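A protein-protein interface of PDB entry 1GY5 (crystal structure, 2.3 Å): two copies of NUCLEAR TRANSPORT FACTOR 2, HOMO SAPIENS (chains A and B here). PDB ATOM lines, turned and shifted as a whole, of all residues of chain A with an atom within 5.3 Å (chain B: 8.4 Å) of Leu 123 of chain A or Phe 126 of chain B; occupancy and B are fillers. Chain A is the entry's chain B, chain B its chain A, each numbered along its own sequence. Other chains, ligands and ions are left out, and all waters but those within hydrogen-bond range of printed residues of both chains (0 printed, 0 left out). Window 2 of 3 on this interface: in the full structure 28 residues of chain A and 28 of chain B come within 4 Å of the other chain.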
ATOM      1  N   MET A  97     -34.351 -22.860  14.169  1.00  0.00           N
ATOM      2  CA  MET A  97     -33.013 -23.008  14.719  1.00  0.00           C
ATOM      3  C   MET A  97     -32.985 -22.821  16.246  1.00  0.00           C
ATOM      4  O   MET A  97     -33.525 -21.849  16.779  1.00  0.00           O
ATOM      5  CB  MET A  97     -32.068 -22.020  14.006  1.00  0.00           C
ATOM      6  CG  MET A  97     -30.578 -22.144  14.372  1.00  0.00           C
ATOM      7  SD  MET A  97     -29.426 -21.715  13.000  1.00  0.00           S
ATOM      8  CE  MET A  97     -30.379 -20.474  12.061  1.00  0.00           C
ATOM      9  N   GLY A  98     -32.375 -23.775  16.945  1.00  0.00           N
ATOM     10  CA  GLY A  98     -32.283 -23.689  18.389  1.00  0.00           C
ATOM     11  C   GLY A  98     -31.296 -22.613  18.801  1.00  0.00           C
ATOM     12  O   GLY A  98     -30.397 -22.278  18.032  1.00  0.00           O
ATOM     13  N   HIS A 100     -29.326 -20.423  22.465  1.00  0.00           N
ATOM     14  CA  HIS A 100     -29.029 -20.282  23.892  1.00  0.00           C
ATOM     15  C   HIS A 100     -28.760 -18.794  24.127  1.00  0.00           C
ATOM     16  O   HIS A 100     -28.144 -18.144  23.293  1.00  0.00           O
ATOM     17  CB  HIS A 100     -27.746 -21.044  24.277  1.00  0.00           C
ATOM     18  CG  HIS A 100     -27.838 -22.532  24.144  1.00  0.00           C
ATOM     19  ND1 HIS A 100     -26.774 -23.363  24.425  1.00  0.00           N
ATOM     20  CD2 HIS A 100     -28.866 -23.344  23.807  1.00  0.00           C
ATOM     21  CE1 HIS A 100     -27.145 -24.622  24.274  1.00  0.00           C
ATOM     22  NE2 HIS A 100     -28.411 -24.639  23.900  1.00  0.00           N
ATOM     23  N   ARG A 120     -25.996 -17.463  21.212  1.00  0.00           N
ATOM     24  CA  ARG A 120     -25.330 -18.453  20.397  1.00  0.00           C
ATOM     25  C   ARG A 120     -26.372 -19.346  19.731  1.00  0.00           C
ATOM     26  O   ARG A 120     -27.392 -19.697  20.329  1.00  0.00           O
ATOM     27  CB  ARG A 120     -24.375 -19.259  21.281  1.00  0.00           C
ATOM     28  CG  ARG A 120     -23.285 -20.007  20.538  1.00  0.00           C
ATOM     29  CD  ARG A 120     -22.176 -20.432  21.502  1.00  0.00           C
ATOM     30  NE  ARG A 120     -21.016 -19.541  21.449  1.00  0.00           N
ATOM     31  CZ  ARG A 120     -20.171 -19.483  20.422  1.00  0.00           C
ATOM     32  NH1 ARG A 120     -20.362 -20.266  19.371  1.00  0.00           N
ATOM     33  NH2 ARG A 120     -19.135 -18.651  20.441  1.00  0.00           N
ATOM     34  N   LEU A 121     -26.113 -19.684  18.473  1.00  0.00           N
ATOM     35  CA  LEU A 121     -27.011 -20.523  17.692  1.00  0.00           C
ATOM     36  C   LEU A 121     -26.567 -21.968  17.696  1.00  0.00           C
ATOM     37  O   LEU A 121     -25.374 -22.259  17.747  1.00  0.00           O
ATOM     38  CB  LEU A 121     -27.063 -20.042  16.248  1.00  0.00           C
ATOM     39  CG  LEU A 121     -27.862 -18.784  15.950  1.00  0.00           C
ATOM     40  CD1 LEU A 121     -27.769 -18.481  14.464  1.00  0.00           C
ATOM     41  CD2 LEU A 121     -29.321 -18.995  16.369  1.00  0.00           C
ATOM     42  N   ALA A 122     -27.538 -22.871  17.635  1.00  0.00           N
ATOM     43  CA  ALA A 122     -27.254 -24.294  17.610  1.00  0.00           C
ATOM     44  C   ALA A 122     -27.232 -24.744  16.158  1.00  0.00           C
ATOM     45  O   ALA A 122     -26.801 -24.005  15.282  1.00  0.00           O
ATOM     46  CB  ALA A 122     -28.322 -25.046  18.374  1.00  0.00           C
ATOM     47  N   LEU A 123     -27.700 -25.965  15.915  1.00  0.00           N
ATOM     48  CA  LEU A 123     -27.767 -26.537  14.568  1.00  0.00           C
ATOM     49  C   LEU A 123     -28.984 -27.461  14.521  1.00  0.00           C
ATOM     50  O   LEU A 123     -29.055 -28.445  15.266  1.00  0.00           O
ATOM     51  CB  LEU A 123     -26.486 -27.319  14.262  1.00  0.00           C
ATOM     52  CG  LEU A 123     -25.188 -26.512  14.374  1.00  0.00           C
ATOM     53  CD1 LEU A 123     -23.987 -27.441  14.363  1.00  0.00           C
ATOM     54  CD2 LEU A 123     -25.113 -25.518  13.232  1.00  0.00           C
ATOM     55  N   HIS A 124     -29.946 -27.124  13.660  1.00  0.00           N
ATOM     56  CA  HIS A 124     -31.188 -27.889  13.508  1.00  0.00           C
ATOM     57  C   HIS A 124     -30.982 -29.398  13.536  1.00  0.00           C
ATOM     58  O   HIS A 124     -31.606 -30.099  14.334  1.00  0.00           O
ATOM     59  CB  HIS A 124     -31.895 -27.486  12.210  1.00  0.00           C
ATOM     60  N   ASN A 125     -30.115 -29.893  12.658  1.00  0.00           N
ATOM     61  CA  ASN A 125     -29.813 -31.323  12.566  1.00  0.00           C
ATOM     62  C   ASN A 125     -31.048 -32.174  12.258  1.00  0.00           C
ATOM     63  O   ASN A 125     -30.932 -33.372  11.965  1.00  0.00           O
ATOM     64  CB  ASN A 125     -29.151 -31.804  13.855  1.00  0.00           C
ATOM     65  N   THR B  69     -16.370 -27.131  23.520  1.00  0.00           N
ATOM     66  CA  THR B  69     -16.616 -26.789  22.119  1.00  0.00           C
ATOM     67  C   THR B  69     -16.343 -25.299  21.904  1.00  0.00           C
ATOM     68  O   THR B  69     -15.604 -24.921  20.995  1.00  0.00           O
ATOM     69  CB  THR B  69     -18.091 -27.076  21.722  1.00  0.00           C
ATOM     70  OG1 THR B  69     -18.314 -28.490  21.677  1.00  0.00           O
ATOM     71  CG2 THR B  69     -18.413 -26.472  20.363  1.00  0.00           C
ATOM     72  N   ALA B  70     -16.950 -24.462  22.743  1.00  0.00           N
ATOM     73  CA  ALA B  70     -16.777 -23.016  22.643  1.00  0.00           C
ATOM     74  C   ALA B  70     -16.990 -22.324  23.985  1.00  0.00           C
ATOM     75  O   ALA B  70     -17.703 -22.829  24.856  1.00  0.00           O
ATOM     76  CB  ALA B  70     -17.741 -22.451  21.624  1.00  0.00           C
ATOM     77  N   ASP B  72     -17.305 -18.137  25.717  1.00  0.00           N
ATOM     78  CA  ASP B  72     -17.318 -16.684  25.573  1.00  0.00           C
ATOM     79  C   ASP B  72     -17.196 -16.063  26.960  1.00  0.00           C
ATOM     80  O   ASP B  72     -17.803 -16.545  27.923  1.00  0.00           O
ATOM     81  CB  ASP B  72     -18.622 -16.220  24.920  1.00  0.00           C
ATOM     82  CG  ASP B  72     -18.830 -16.815  23.552  1.00  0.00           C
ATOM     83  OD1 ASP B  72     -17.951 -16.632  22.691  1.00  0.00           O
ATOM     84  OD2 ASP B  72     -19.872 -17.463  23.334  1.00  0.00           O
ATOM     85  N   MET B  84     -19.576 -18.271  29.330  1.00  0.00           N
ATOM     86  CA  MET B  84     -20.577 -19.185  28.807  1.00  0.00           C
ATOM     87  C   MET B  84     -19.840 -20.249  28.015  1.00  0.00           C
ATOM     88  O   MET B  84     -19.035 -19.939  27.148  1.00  0.00           O
ATOM     89  CB  MET B  84     -21.590 -18.461  27.920  1.00  0.00           C
ATOM     90  CG  MET B  84     -22.758 -19.351  27.550  1.00  0.00           C
ATOM     91  SD  MET B  84     -24.357 -18.521  27.537  1.00  0.00           S
ATOM     92  CE  MET B  84     -24.610 -18.320  25.737  1.00  0.00           C
ATOM     93  N   VAL B  85     -20.112 -21.506  28.344  1.00  0.00           N
ATOM     94  CA  VAL B  85     -19.460 -22.636  27.702  1.00  0.00           C
ATOM     95  C   VAL B  85     -20.424 -23.563  26.950  1.00  0.00           C
ATOM     96  O   VAL B  85     -21.572 -23.751  27.356  1.00  0.00           O
ATOM     97  CB  VAL B  85     -18.706 -23.488  28.762  1.00  0.00           C
ATOM     98  CG1 VAL B  85     -18.051 -24.693  28.100  1.00  0.00           C
ATOM     99  CG2 VAL B  85     -17.666 -22.632  29.487  1.00  0.00           C
ATOM    100  N   VAL B  86     -19.934 -24.133  25.854  1.00  0.00           N
ATOM    101  CA  VAL B  86     -20.687 -25.091  25.051  1.00  0.00           C
ATOM    102  C   VAL B  86     -19.709 -26.230  24.793  1.00  0.00           C
ATOM    103  O   VAL B  86     -18.533 -25.988  24.530  1.00  0.00           O
ATOM    104  CB  VAL B  86     -21.136 -24.504  23.694  1.00  0.00           C
ATOM    105  CG1 VAL B  86     -21.585 -25.630  22.762  1.00  0.00           C
ATOM    106  CG2 VAL B  86     -22.291 -23.537  23.909  1.00  0.00           C
ATOM    107  N   GLY B  87     -20.183 -27.466  24.881  1.00  0.00           N
ATOM    108  CA  GLY B  87     -19.303 -28.593  24.658  1.00  0.00           C
ATOM    109  C   GLY B  87     -20.003 -29.924  24.839  1.00  0.00           C
ATOM    110  O   GLY B  87     -21.232 -29.997  24.887  1.00  0.00           O
ATOM    111  N   GLN B  88     -19.218 -30.986  24.952  1.00  0.00           N
ATOM    112  CA  GLN B  88     -19.784 -32.313  25.115  1.00  0.00           C
ATOM    113  C   GLN B  88     -19.258 -32.958  26.382  1.00  0.00           C
ATOM    114  O   GLN B  88     -18.227 -32.555  26.917  1.00  0.00           O
ATOM    115  CB  GLN B  88     -19.409 -33.198  23.922  1.00  0.00           C
ATOM    116  CG  GLN B  88     -19.740 -32.630  22.560  1.00  0.00           C
ATOM    117  CD  GLN B  88     -19.304 -33.560  21.439  1.00  0.00           C
ATOM    118  OE1 GLN B  88     -18.128 -33.914  21.337  1.00  0.00           O
ATOM    119  NE2 GLN B  88     -20.251 -33.965  20.595  1.00  0.00           N
ATOM    120  N   GLY B  98     -24.514 -33.461  24.912  1.00  0.00           N
ATOM    121  CA  GLY B  98     -24.206 -32.058  24.699  1.00  0.00           C
ATOM    122  C   GLY B  98     -24.514 -31.288  25.966  1.00  0.00           C
ATOM    123  O   GLY B  98     -25.159 -31.823  26.863  1.00  0.00           O
ATOM    124  N   PHE B  99     -24.066 -30.039  26.055  1.00  0.00           N
ATOM    125  CA  PHE B  99     -24.327 -29.253  27.254  1.00  0.00           C
ATOM    126  C   PHE B  99     -23.862 -27.808  27.150  1.00  0.00           C
ATOM    127  O   PHE B  99     -22.968 -27.486  26.369  1.00  0.00           O
ATOM    128  CB  PHE B  99     -23.623 -29.897  28.467  1.00  0.00           C
ATOM    129  CG  PHE B  99     -22.195 -29.436  28.671  1.00  0.00           C
ATOM    130  CD1 PHE B  99     -21.916 -28.247  29.353  1.00  0.00           C
ATOM    131  CD2 PHE B  99     -21.129 -30.178  28.172  1.00  0.00           C
ATOM    132  CE1 PHE B  99     -20.598 -27.809  29.532  1.00  0.00           C
ATOM    133  CE2 PHE B  99     -19.812 -29.751  28.343  1.00  0.00           C
ATOM    134  CZ  PHE B  99     -19.548 -28.559  29.028  1.00  0.00           C
ATOM    135  N   HIS B 100     -24.487 -26.944  27.939  1.00  0.00           N
ATOM    136  CA  HIS B 100     -24.069 -25.559  28.022  1.00  0.00           C
ATOM    137  C   HIS B 100     -24.050 -25.182  29.503  1.00  0.00           C
ATOM    138  O   HIS B 100     -24.902 -25.616  30.281  1.00  0.00           O
ATOM    139  CB  HIS B 100     -24.963 -24.616  27.207  1.00  0.00           C
ATOM    140  CG  HIS B 100     -26.396 -24.583  27.631  1.00  0.00           C
ATOM    141  ND1 HIS B 100     -27.322 -25.509  27.197  1.00  0.00           N
ATOM    142  CD2 HIS B 100     -27.084 -23.679  28.368  1.00  0.00           C
ATOM    143  CE1 HIS B 100     -28.519 -25.171  27.644  1.00  0.00           C
ATOM    144  NE2 HIS B 100     -28.402 -24.065  28.357  1.00  0.00           N
ATOM    145  N   ALA B 122     -27.825 -30.774  26.416  1.00  0.00           N
ATOM    146  CA  ALA B 122     -28.253 -30.345  25.094  1.00  0.00           C
ATOM    147  C   ALA B 122     -28.174 -31.496  24.116  1.00  0.00           C
ATOM    148  O   ALA B 122     -27.231 -32.283  24.150  1.00  0.00           O
ATOM    149  CB  ALA B 122     -27.382 -29.184  24.609  1.00  0.00           C
ATOM    150  N   LEU B 123     -29.178 -31.588  23.248  1.00  0.00           N
ATOM    151  CA  LEU B 123     -29.241 -32.637  22.240  1.00  0.00           C
ATOM    152  C   LEU B 123     -28.746 -32.125  20.895  1.00  0.00           C
ATOM    153  O   LEU B 123     -28.553 -32.899  19.957  1.00  0.00           O
ATOM    154  CB  LEU B 123     -30.672 -33.141  22.088  1.00  0.00           C
ATOM    155  CG  LEU B 123     -31.242 -33.907  23.272  1.00  0.00           C
ATOM    156  CD1 LEU B 123     -32.643 -34.374  22.938  1.00  0.00           C
ATOM    157  CD2 LEU B 123     -30.339 -35.091  23.589  1.00  0.00           C
ATOM    158  N   HIS B 124     -28.555 -30.816  20.795  1.00  0.00           N
ATOM    159  CA  HIS B 124     -28.082 -30.228  19.553  1.00  0.00           C
ATOM    160  C   HIS B 124     -26.644 -29.760  19.744  1.00  0.00           C
ATOM    161  O   HIS B 124     -26.248 -29.419  20.854  1.00  0.00           O
ATOM    162  CB  HIS B 124     -29.011 -29.079  19.148  1.00  0.00           C
ATOM    163  CG  HIS B 124     -30.408 -29.530  18.833  1.00  0.00           C
ATOM    164  ND1 HIS B 124     -30.766 -30.047  17.604  1.00  0.00           N
ATOM    165  CD2 HIS B 124     -31.515 -29.611  19.610  1.00  0.00           C
ATOM    166  CE1 HIS B 124     -32.030 -30.428  17.639  1.00  0.00           C
ATOM    167  NE2 HIS B 124     -32.509 -30.175  18.846  1.00  0.00           N
ATOM    168  N   ASN B 125     -25.862 -29.776  18.667  1.00  0.00           N
ATOM    169  CA  ASN B 125     -24.472 -29.365  18.754  1.00  0.00           C
ATOM    170  C   ASN B 125     -24.202 -27.959  18.248  1.00  0.00           C
ATOM    171  O   ASN B 125     -25.120 -27.250  17.825  1.00  0.00           O
ATOM    172  N   PHE B 126     -22.932 -27.558  18.301  1.00  0.00           N
ATOM    173  CA  PHE B 126     -22.494 -26.237  17.848  1.00  0.00           C
ATOM    174  C   PHE B 126     -21.280 -26.368  16.933  1.00  0.00           C
ATOM    175  O   PHE B 126     -20.831 -27.513  16.715  1.00  0.00           O
ATOM    176  CB  PHE B 126     -22.142 -25.344  19.047  1.00  0.00           C
ATOM    177  CG  PHE B 126     -23.337 -24.905  19.847  1.00  0.00           C
ATOM    178  CD1 PHE B 126     -24.178 -25.842  20.449  1.00  0.00           C
ATOM    179  CD2 PHE B 126     -23.635 -23.554  19.985  1.00  0.00           C
ATOM    180  CE1 PHE B 126     -25.303 -25.436  21.174  1.00  0.00           C
ATOM    181  CE2 PHE B 126     -24.754 -23.138  20.708  1.00  0.00           C
ATOM    182  CZ  PHE B 126     -25.589 -24.083  21.302  1.00  0.00           C
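The backbone NH (N) of Ala 122 of chain A sits at hydrogen-bond distance from the backbone carbonyl oxygen (O) of Gly 98 of chain A, at 2.9 Å.
The backbone NH (N) of His 100 of chain A sits at hydrogen-bond distance from the backbone carbonyl oxygen (O) of Arg 120 of chain A (3.0 Å).
The backbone NH (N) of Thr 69 of chain B is in hydrogen-bond range of the backbone carbonyl oxygen (O) of Val 86 of chain B (2.6 Å).
O of Asp 72 of chain B lies within hydrogen-bond range of N of Met 84 of chain B.
O of Ala 70 of chain B sits at hydrogen-bond distance from N of Val 86 of chain B (2.8 Å).
ND1 of His 100 of chain B touches CE1 of His 100 of chain A (3.1 Å).
CZ of Phe 126 of chain B touches CE1 of His 100 of chain A (3.4 Å).
CG2 of Val 86 of chain B touches CD of Arg 120 of chain A (3.9 Å).
Arg 120 of chain A touches Phe 126 of chain B.
Phe 126 of chain B touches Leu 121 of chain A (CD2 to O, 3.1 Å).
Asn 125 of chain B touches Ala 122 of chain A.
Phe 126 of chain B touches Leu 123 of chain A (C to CD1, 3.9 Å).
A ring nitrogen (ND1) of His 124 of chain B lies close to the backbone carbonyl oxygen of His 124 of chain A (3.4 Å).
The backbone carbonyl oxygen of Leu 123 of chain A sits at hydrogen-bond distance from a ring nitrogen (ND1) of His 124 of chain B.
The guanidinium group (NE) of Arg 120 of chain A lies within salt-bridge range of the side-chain carboxylate (OD2) of Asp 72 of chain B (3.0 Å).
The backbone carbonyl oxygen of Asn 125 of chain B lies within hydrogen-bond range of the backbone NH of Leu 123 of chain A (3.5 Å).
Leu 123 of chain A touches just these residues of chain B: His 124, Asn 125 and Phe 126.
Phe 126 of chain B touches four residues of chain A.
Ala 122 of chain A touches just one residue of chain B: Asn 125.
His 124 of chain A touches just one residue of chain B: His 124.
Of the printed residues of chain B, His 100 of chain A touches His 100 and Phe 126.
Of the printed residues of chain B, Leu 121 of chain A touches Phe 126.
Printed residues of chain A within 4 Å of His 100 of chain B: His 100.
Thr 69 of chain B touches none of the printed residues of chain A.
The nearest residue of chain B that does not touch Leu 123 of chain A is Leu 123 of chain B (6.5 Å).
The nearest residue of chain A that does not touch Phe 126 of chain B is Ala 122 of chain A (4.1 Å).
The nearest printed residue of chain A that does not touch Asp 72 of chain B is Leu 121 of chain A (8.2 Å).
His 100 of chain B touches its own counterpart, His 100 of chain A.
Leu 123 of chain A touches His 124 of chain B, but with the chains exchanged His 124 of chain A does not touch Leu 123 of chain B (7.0 Å).
Leu 123 of chain A touches Asn 125 of chain B, but with the chains exchanged Asn 125 of chain A does not touch Leu 123 of chain B (6.2 Å).
His 124 of chain A touches its own counterpart, His 124 of chain B.
Of the 11 pairs that touch across the chains among the printed residues, 2 have their exchanged pair printed and touching as well.
Hydrophobic or aromatic side chains of chain B within 4 Å of the printed part of chain A: Val 86, His 100, His 124 and Phe 126.
Hydrophobic or aromatic side chains of chain A that line the printed part of chain B: His 100, Ala 122 and Leu 123.
Among the printed residues, Asp or Glu carboxylates within 4 Å of a Lys or Arg side-chain nitrogen of the other chain: Arg 120 of chain A with Asp 72 of chain B.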
